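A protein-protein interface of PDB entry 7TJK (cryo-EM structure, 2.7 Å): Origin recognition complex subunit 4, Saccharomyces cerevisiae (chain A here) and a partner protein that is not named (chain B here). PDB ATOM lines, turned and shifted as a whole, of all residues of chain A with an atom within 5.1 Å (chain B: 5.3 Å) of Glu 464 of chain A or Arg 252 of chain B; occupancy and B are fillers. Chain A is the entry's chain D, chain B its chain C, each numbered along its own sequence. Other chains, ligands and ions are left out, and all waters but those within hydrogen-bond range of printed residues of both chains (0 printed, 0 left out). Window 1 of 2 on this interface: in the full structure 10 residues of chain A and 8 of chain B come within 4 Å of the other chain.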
ATOM      1  N   VAL A 459      -9.109   3.490 -30.324  1.00  0.00           N
ATOM      2  CA  VAL A 459      -7.756   3.064 -29.982  1.00  0.00           C
ATOM      3  C   VAL A 459      -7.636   2.851 -28.464  1.00  0.00           C
ATOM      4  O   VAL A 459      -6.750   2.119 -28.000  1.00  0.00           O
ATOM      5  CB  VAL A 459      -6.768   4.095 -30.581  1.00  0.00           C
ATOM      6  CG1 VAL A 459      -5.330   3.955 -30.099  1.00  0.00           C
ATOM      7  CG2 VAL A 459      -6.766   3.979 -32.095  1.00  0.00           C
ATOM      8  N   LYS A 460      -8.570   3.419 -27.688  1.00  0.00           N
ATOM      9  CA  LYS A 460      -8.611   3.226 -26.235  1.00  0.00           C
ATOM     10  C   LYS A 460      -8.778   1.758 -25.842  1.00  0.00           C
ATOM     11  O   LYS A 460      -8.119   1.276 -24.910  1.00  0.00           O
ATOM     12  CB  LYS A 460      -9.751   4.059 -25.648  1.00  0.00           C
ATOM     13  CG  LYS A 460      -9.996   3.862 -24.165  1.00  0.00           C
ATOM     14  CD  LYS A 460     -11.186   4.674 -23.700  1.00  0.00           C
ATOM     15  CE  LYS A 460     -11.568   4.334 -22.274  1.00  0.00           C
ATOM     16  NZ  LYS A 460     -10.517   4.752 -21.312  1.00  0.00           N
ATOM     17  N   ASN A 461      -9.645   1.031 -26.553  1.00  0.00           N
ATOM     18  CA  ASN A 461      -9.856  -0.387 -26.269  1.00  0.00           C
ATOM     19  C   ASN A 461      -8.612  -1.210 -26.591  1.00  0.00           C
ATOM     20  O   ASN A 461      -8.249  -2.121 -25.837  1.00  0.00           O
ATOM     21  CB  ASN A 461     -11.068  -0.887 -27.055  1.00  0.00           C
ATOM     22  CG  ASN A 461     -11.216  -2.391 -27.015  1.00  0.00           C
ATOM     23  OD1 ASN A 461     -10.996  -3.075 -28.012  1.00  0.00           O
ATOM     24  ND2 ASN A 461     -11.603  -2.916 -25.860  1.00  0.00           N
ATOM     25  N   VAL A 462      -7.942  -0.882 -27.700  1.00  0.00           N
ATOM     26  CA  VAL A 462      -6.679  -1.516 -28.078  1.00  0.00           C
ATOM     27  C   VAL A 462      -5.610  -1.265 -27.020  1.00  0.00           C
ATOM     28  O   VAL A 462      -4.849  -2.171 -26.650  1.00  0.00           O
ATOM     29  CB  VAL A 462      -6.250  -1.002 -29.466  1.00  0.00           C
ATOM     30  CG1 VAL A 462      -4.837  -1.419 -29.809  1.00  0.00           C
ATOM     31  CG2 VAL A 462      -7.214  -1.504 -30.521  1.00  0.00           C
ATOM     32  N   TRP A 463      -5.563  -0.036 -26.500  1.00  0.00           N
ATOM     33  CA  TRP A 463      -4.626   0.328 -25.442  1.00  0.00           C
ATOM     34  C   TRP A 463      -4.887  -0.464 -24.166  1.00  0.00           C
ATOM     35  O   TRP A 463      -3.947  -0.935 -23.511  1.00  0.00           O
ATOM     36  CB  TRP A 463      -4.736   1.826 -25.174  1.00  0.00           C
ATOM     37  CG  TRP A 463      -3.692   2.379 -24.278  1.00  0.00           C
ATOM     38  CD1 TRP A 463      -3.780   2.572 -22.933  1.00  0.00           C
ATOM     39  CD2 TRP A 463      -2.396   2.834 -24.666  1.00  0.00           C
ATOM     40  NE1 TRP A 463      -2.613   3.115 -22.457  1.00  0.00           N
ATOM     41  CE2 TRP A 463      -1.749   3.289 -23.504  1.00  0.00           C
ATOM     42  CE3 TRP A 463      -1.721   2.902 -25.886  1.00  0.00           C
ATOM     43  CZ2 TRP A 463      -0.458   3.800 -23.526  1.00  0.00           C
ATOM     44  CZ3 TRP A 463      -0.446   3.411 -25.906  1.00  0.00           C
ATOM     45  CH2 TRP A 463       0.175   3.853 -24.734  1.00  0.00           C
ATOM     46  N   GLU A 464      -6.162  -0.628 -23.804  1.00  0.00           N
ATOM     47  CA  GLU A 464      -6.510  -1.396 -22.614  1.00  0.00           C
ATOM     48  C   GLU A 464      -6.185  -2.878 -22.773  1.00  0.00           C
ATOM     49  O   GLU A 464      -5.751  -3.519 -21.808  1.00  0.00           O
ATOM     50  CB  GLU A 464      -7.986  -1.188 -22.279  1.00  0.00           C
ATOM     51  CG  GLU A 464      -8.243   0.144 -21.597  1.00  0.00           C
ATOM     52  CD  GLU A 464      -9.682   0.602 -21.693  1.00  0.00           C
ATOM     53  OE1 GLU A 464     -10.464  -0.019 -22.442  1.00  0.00           O
ATOM     54  OE2 GLU A 464     -10.025   1.602 -21.029  1.00  0.00           O
ATOM     55  N   ASN A 465      -6.372  -3.434 -23.976  1.00  0.00           N
ATOM     56  CA  ASN A 465      -5.961  -4.817 -24.220  1.00  0.00           C
ATOM     57  C   ASN A 465      -4.444  -4.974 -24.182  1.00  0.00           C
ATOM     58  O   ASN A 465      -3.939  -6.012 -23.740  1.00  0.00           O
ATOM     59  CB  ASN A 465      -6.511  -5.321 -25.553  1.00  0.00           C
ATOM     60  CG  ASN A 465      -8.008  -5.170 -25.661  1.00  0.00           C
ATOM     61  OD1 ASN A 465      -8.683  -4.847 -24.685  1.00  0.00           O
ATOM     62  ND2 ASN A 465      -8.539  -5.394 -26.854  1.00  0.00           N
ATOM     63  N   LEU A 466      -3.703  -3.969 -24.656  1.00  0.00           N
ATOM     64  CA  LEU A 466      -2.245  -4.037 -24.584  1.00  0.00           C
ATOM     65  C   LEU A 466      -1.743  -3.931 -23.151  1.00  0.00           C
ATOM     66  O   LEU A 466      -0.713  -4.526 -22.813  1.00  0.00           O
ATOM     67  CB  LEU A 466      -1.613  -2.942 -25.443  1.00  0.00           C
ATOM     68  CG  LEU A 466      -1.606  -3.177 -26.954  1.00  0.00           C
ATOM     69  CD1 LEU A 466      -1.140  -1.930 -27.683  1.00  0.00           C
ATOM     70  CD2 LEU A 466      -0.742  -4.371 -27.313  1.00  0.00           C
ATOM     71  N   VAL A 467      -2.434  -3.164 -22.308  1.00  0.00           N
ATOM     72  CA  VAL A 467      -2.110  -3.150 -20.884  1.00  0.00           C
ATOM     73  C   VAL A 467      -2.447  -4.498 -20.248  1.00  0.00           C
ATOM     74  O   VAL A 467      -1.683  -5.022 -19.427  1.00  0.00           O
ATOM     75  CB  VAL A 467      -2.830  -1.975 -20.192  1.00  0.00           C
ATOM     76  CG1 VAL A 467      -2.715  -2.059 -18.675  1.00  0.00           C
ATOM     77  CG2 VAL A 467      -2.261  -0.655 -20.680  1.00  0.00           C
ATOM     78  N   GLN A 468      -3.571  -5.099 -20.654  1.00  0.00           N
ATOM     79  CA  GLN A 468      -4.006  -6.380 -20.101  1.00  0.00           C
ATOM     80  C   GLN A 468      -3.062  -7.524 -20.469  1.00  0.00           C
ATOM     81  O   GLN A 468      -2.828  -8.421 -19.651  1.00  0.00           O
ATOM     82  CB  GLN A 468      -5.430  -6.678 -20.576  1.00  0.00           C
ATOM     83  CG  GLN A 468      -6.019  -7.994 -20.097  1.00  0.00           C
ATOM     84  CD  GLN A 468      -6.235  -8.026 -18.599  1.00  0.00           C
ATOM     85  OE1 GLN A 468      -6.823  -7.109 -18.026  1.00  0.00           O
ATOM     86  NE2 GLN A 468      -5.759  -9.085 -17.954  1.00  0.00           N
ATOM     87  N   ASP B 217     -14.609   0.249 -11.011  1.00  0.00           N
ATOM     88  CA  ASP B 217     -14.533  -0.622 -12.179  1.00  0.00           C
ATOM     89  C   ASP B 217     -14.332  -2.081 -11.774  1.00  0.00           C
ATOM     90  O   ASP B 217     -15.083  -2.963 -12.216  1.00  0.00           O
ATOM     91  CB  ASP B 217     -13.393  -0.144 -13.080  1.00  0.00           C
ATOM     92  CG  ASP B 217     -13.550  -0.587 -14.513  1.00  0.00           C
ATOM     93  OD1 ASP B 217     -14.508  -1.321 -14.803  1.00  0.00           O
ATOM     94  OD2 ASP B 217     -12.715  -0.194 -15.354  1.00  0.00           O
ATOM     95  N   ASN B 218     -13.363  -2.337 -10.888  1.00  0.00           N
ATOM     96  CA  ASN B 218     -13.111  -3.696 -10.421  1.00  0.00           C
ATOM     97  C   ASN B 218     -14.286  -4.248  -9.625  1.00  0.00           C
ATOM     98  O   ASN B 218     -14.573  -5.446  -9.707  1.00  0.00           O
ATOM     99  CB  ASN B 218     -11.830  -3.738  -9.590  1.00  0.00           C
ATOM    100  CG  ASN B 218     -10.610  -3.293 -10.375  1.00  0.00           C
ATOM    101  OD1 ASN B 218     -10.529  -3.486 -11.586  1.00  0.00           O
ATOM    102  ND2 ASN B 218      -9.653  -2.688  -9.683  1.00  0.00           N
ATOM    103  N   ILE B 221     -16.853  -5.430 -12.460  1.00  0.00           N
ATOM    104  CA  ILE B 221     -16.512  -6.777 -12.958  1.00  0.00           C
ATOM    105  C   ILE B 221     -16.656  -7.846 -11.861  1.00  0.00           C
ATOM    106  O   ILE B 221     -17.060  -8.982 -12.150  1.00  0.00           O
ATOM    107  CB  ILE B 221     -15.129  -6.829 -13.676  1.00  0.00           C
ATOM    108  CG1 ILE B 221     -15.085  -5.989 -14.964  1.00  0.00           C
ATOM    109  CG2 ILE B 221     -14.666  -8.237 -14.053  1.00  0.00           C
ATOM    110  CD1 ILE B 221     -14.693  -4.588 -14.891  1.00  0.00           C
ATOM    111  N   ASN B 250     -13.306   7.251 -17.767  1.00  0.00           N
ATOM    112  CA  ASN B 250     -12.600   6.723 -16.609  1.00  0.00           C
ATOM    113  C   ASN B 250     -12.815   5.231 -16.417  1.00  0.00           C
ATOM    114  O   ASN B 250     -12.000   4.583 -15.753  1.00  0.00           O
ATOM    115  CB  ASN B 250     -13.031   7.471 -15.345  1.00  0.00           C
ATOM    116  CG  ASN B 250     -12.404   8.842 -15.239  1.00  0.00           C
ATOM    117  OD1 ASN B 250     -11.325   9.001 -14.667  1.00  0.00           O
ATOM    118  ND2 ASN B 250     -13.071   9.844 -15.793  1.00  0.00           N
ATOM    119  N   LEU B 251     -13.889   4.679 -16.966  1.00  0.00           N
ATOM    120  CA  LEU B 251     -14.104   3.242 -16.970  1.00  0.00           C
ATOM    121  C   LEU B 251     -13.478   2.628 -18.216  1.00  0.00           C
ATOM    122  O   LEU B 251     -13.226   3.306 -19.214  1.00  0.00           O
ATOM    123  CB  LEU B 251     -15.596   2.913 -16.917  1.00  0.00           C
ATOM    124  CG  LEU B 251     -16.400   3.360 -15.694  1.00  0.00           C
ATOM    125  CD1 LEU B 251     -17.780   2.727 -15.715  1.00  0.00           C
ATOM    126  CD2 LEU B 251     -15.680   3.023 -14.402  1.00  0.00           C
ATOM    127  N   ARG B 252     -13.224   1.326 -18.147  1.00  0.00           N
ATOM    128  CA  ARG B 252     -12.675   0.628 -19.295  1.00  0.00           C
ATOM    129  C   ARG B 252     -13.775   0.305 -20.302  1.00  0.00           C
ATOM    130  O   ARG B 252     -14.968   0.343 -19.992  1.00  0.00           O
ATOM    131  CB  ARG B 252     -11.944  -0.640 -18.856  1.00  0.00           C
ATOM    132  CG  ARG B 252     -10.573  -0.360 -18.265  1.00  0.00           C
ATOM    133  CD  ARG B 252      -9.907  -1.618 -17.744  1.00  0.00           C
ATOM    134  NE  ARG B 252     -10.615  -2.184 -16.602  1.00  0.00           N
ATOM    135  CZ  ARG B 252     -10.188  -3.227 -15.903  1.00  0.00           C
ATOM    136  NH1 ARG B 252      -9.053  -3.840 -16.201  1.00  0.00           N
ATOM    137  NH2 ARG B 252     -10.914  -3.662 -14.878  1.00  0.00           N
ATOM    138  N   GLN B 253     -13.350  -0.006 -21.530  1.00  0.00           N
ATOM    139  CA  GLN B 253     -14.287  -0.175 -22.637  1.00  0.00           C
ATOM    140  C   GLN B 253     -15.125  -1.438 -22.488  1.00  0.00           C
ATOM    141  O   GLN B 253     -16.286  -1.463 -22.917  1.00  0.00           O
ATOM    142  CB  GLN B 253     -13.526  -0.198 -23.964  1.00  0.00           C
ATOM    143  CG  GLN B 253     -13.393   1.160 -24.639  1.00  0.00           C
ATOM    144  CD  GLN B 253     -14.616   1.564 -25.446  1.00  0.00           C
ATOM    145  OE1 GLN B 253     -15.658   0.912 -25.405  1.00  0.00           O
ATOM    146  NE2 GLN B 253     -14.488   2.659 -26.186  1.00  0.00           N
ATOM    147  N   SER B 254     -14.558  -2.486 -21.889  1.00  0.00           N
ATOM    148  CA  SER B 254     -15.335  -3.682 -21.585  1.00  0.00           C
ATOM    149  C   SER B 254     -16.407  -3.401 -20.539  1.00  0.00           C
ATOM    150  O   SER B 254     -17.506  -3.960 -20.619  1.00  0.00           O
ATOM    151  CB  SER B 254     -14.404  -4.800 -21.122  1.00  0.00           C
ATOM    152  OG  SER B 254     -13.692  -4.420 -19.958  1.00  0.00           O
ATOM    153  N   THR B 255     -16.112  -2.528 -19.570  1.00  0.00           N
ATOM    154  CA  THR B 255     -17.113  -2.111 -18.590  1.00  0.00           C
ATOM    155  C   THR B 255     -18.241  -1.321 -19.246  1.00  0.00           C
ATOM    156  O   THR B 255     -19.413  -1.495 -18.892  1.00  0.00           O
ATOM    157  CB  THR B 255     -16.449  -1.284 -17.487  1.00  0.00           C
ATOM    158  OG1 THR B 255     -15.317  -1.996 -16.972  1.00  0.00           O
ATOM    159  CG2 THR B 255     -17.421  -1.009 -16.342  1.00  0.00           C
ATOM    160  N   ILE B 256     -17.902  -0.449 -20.201  1.00  0.00           N
ATOM    161  CA  ILE B 256     -18.910   0.309 -20.940  1.00  0.00           C
ATOM    162  C   ILE B 256     -19.779  -0.623 -21.778  1.00  0.00           C
ATOM    163  O   ILE B 256     -21.005  -0.466 -21.833  1.00  0.00           O
ATOM    164  CB  ILE B 256     -18.230   1.391 -21.802  1.00  0.00           C
ATOM    165  CG1 ILE B 256     -17.435   2.357 -20.923  1.00  0.00           C
ATOM    166  CG2 ILE B 256     -19.254   2.162 -22.632  1.00  0.00           C
ATOM    167  CD1 ILE B 256     -18.281   3.115 -19.924  1.00  0.00           C
ATOM    168  N   ARG B 257     -19.161  -1.615 -22.429  1.00  0.00           N
ATOM    169  CA  ARG B 257     -19.916  -2.603 -23.197  1.00  0.00           C
ATOM    170  C   ARG B 257     -20.792  -3.471 -22.301  1.00  0.00           C
ATOM    171  O   ARG B 257     -21.861  -3.919 -22.728  1.00  0.00           O
ATOM    172  CB  ARG B 257     -18.958  -3.477 -24.005  1.00  0.00           C
ATOM    173  CG  ARG B 257     -18.405  -2.808 -25.245  1.00  0.00           C
ATOM    174  CD  ARG B 257     -17.716  -3.807 -26.158  1.00  0.00           C
ATOM    175  NE  ARG B 257     -16.583  -4.452 -25.502  1.00  0.00           N
ATOM    176  CZ  ARG B 257     -15.338  -4.000 -25.544  1.00  0.00           C
ATOM    177  NH1 ARG B 257     -15.028  -2.887 -26.187  1.00  0.00           N
ATOM    178  NH2 ARG B 257     -14.380  -4.680 -24.923  1.00  0.00           N
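The side-chain carboxylate (OD2) of Asp 217 of chain B lies within salt-bridge range of the guanidinium group (NE) of Arg 252 of chain B. OD1 of Asn 218 of chain B is in hydrogen-bond range of NH2 of Arg 252 of chain B, at 3.3 Å. The side-chain amino group (NZ) of Lys 460 of chain A lies within salt-bridge range of the side-chain carboxylate (OE2) of Glu 464 of chain A. The backbone carbonyl oxygen of Asn 461 of chain A lies close to the side-chain amide oxygen of Asn 465 of chain A, at 3.0 Å.
N of Gln 253 of chain B lies within hydrogen-bond range of OE1 of Glu 464 of chain A, at 3.0 Å. The guanidinium group (NH2) of Arg 257 of chain B lies close to the side-chain amide nitrogen (ND2) of Asn 461 of chain A, 3.4 Å away.
Lys 460 of chain A touches Leu 251 of chain B (CE to O, 3.6 Å). ND2 of Asn 461 of chain A touches CB of Gln 253 of chain B, at 3.8 Å. Arg 252 of chain B touches Glu 464 of chain A.
Printed residues of chain B within 4 Å of Lys 460 of chain A: Leu 251. Printed residues of chain B within 4 Å of Asn 461 of chain A: Gln 253 (3.8 Å) and Arg 257 (3.4 Å). Printed residues of chain B within 4 Å of Glu 464 of chain A: Arg 252 (3.3 Å) and Gln 253 (3.0 Å). Printed residues of chain A within 4 Å of Leu 251 of chain B: Lys 460 (3.6 Å). Arg 252 of chain B touches one residue of chain A. Printed residues of chain A within 4 Å of Gln 253 of chain B: Asn 461 and Glu 464. Thr 255 of chain B touches none of the printed residues of chain A. The nearest residue of chain A that does not touch Arg 252 of chain B is Gln 468 of chain A (4.4 Å). The nearest printed residue of chain A that does not touch Arg 257 of chain B is Asn 465 of chain A (5.7 Å).
Among the printed residues, 5 pairs touch across the chains.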
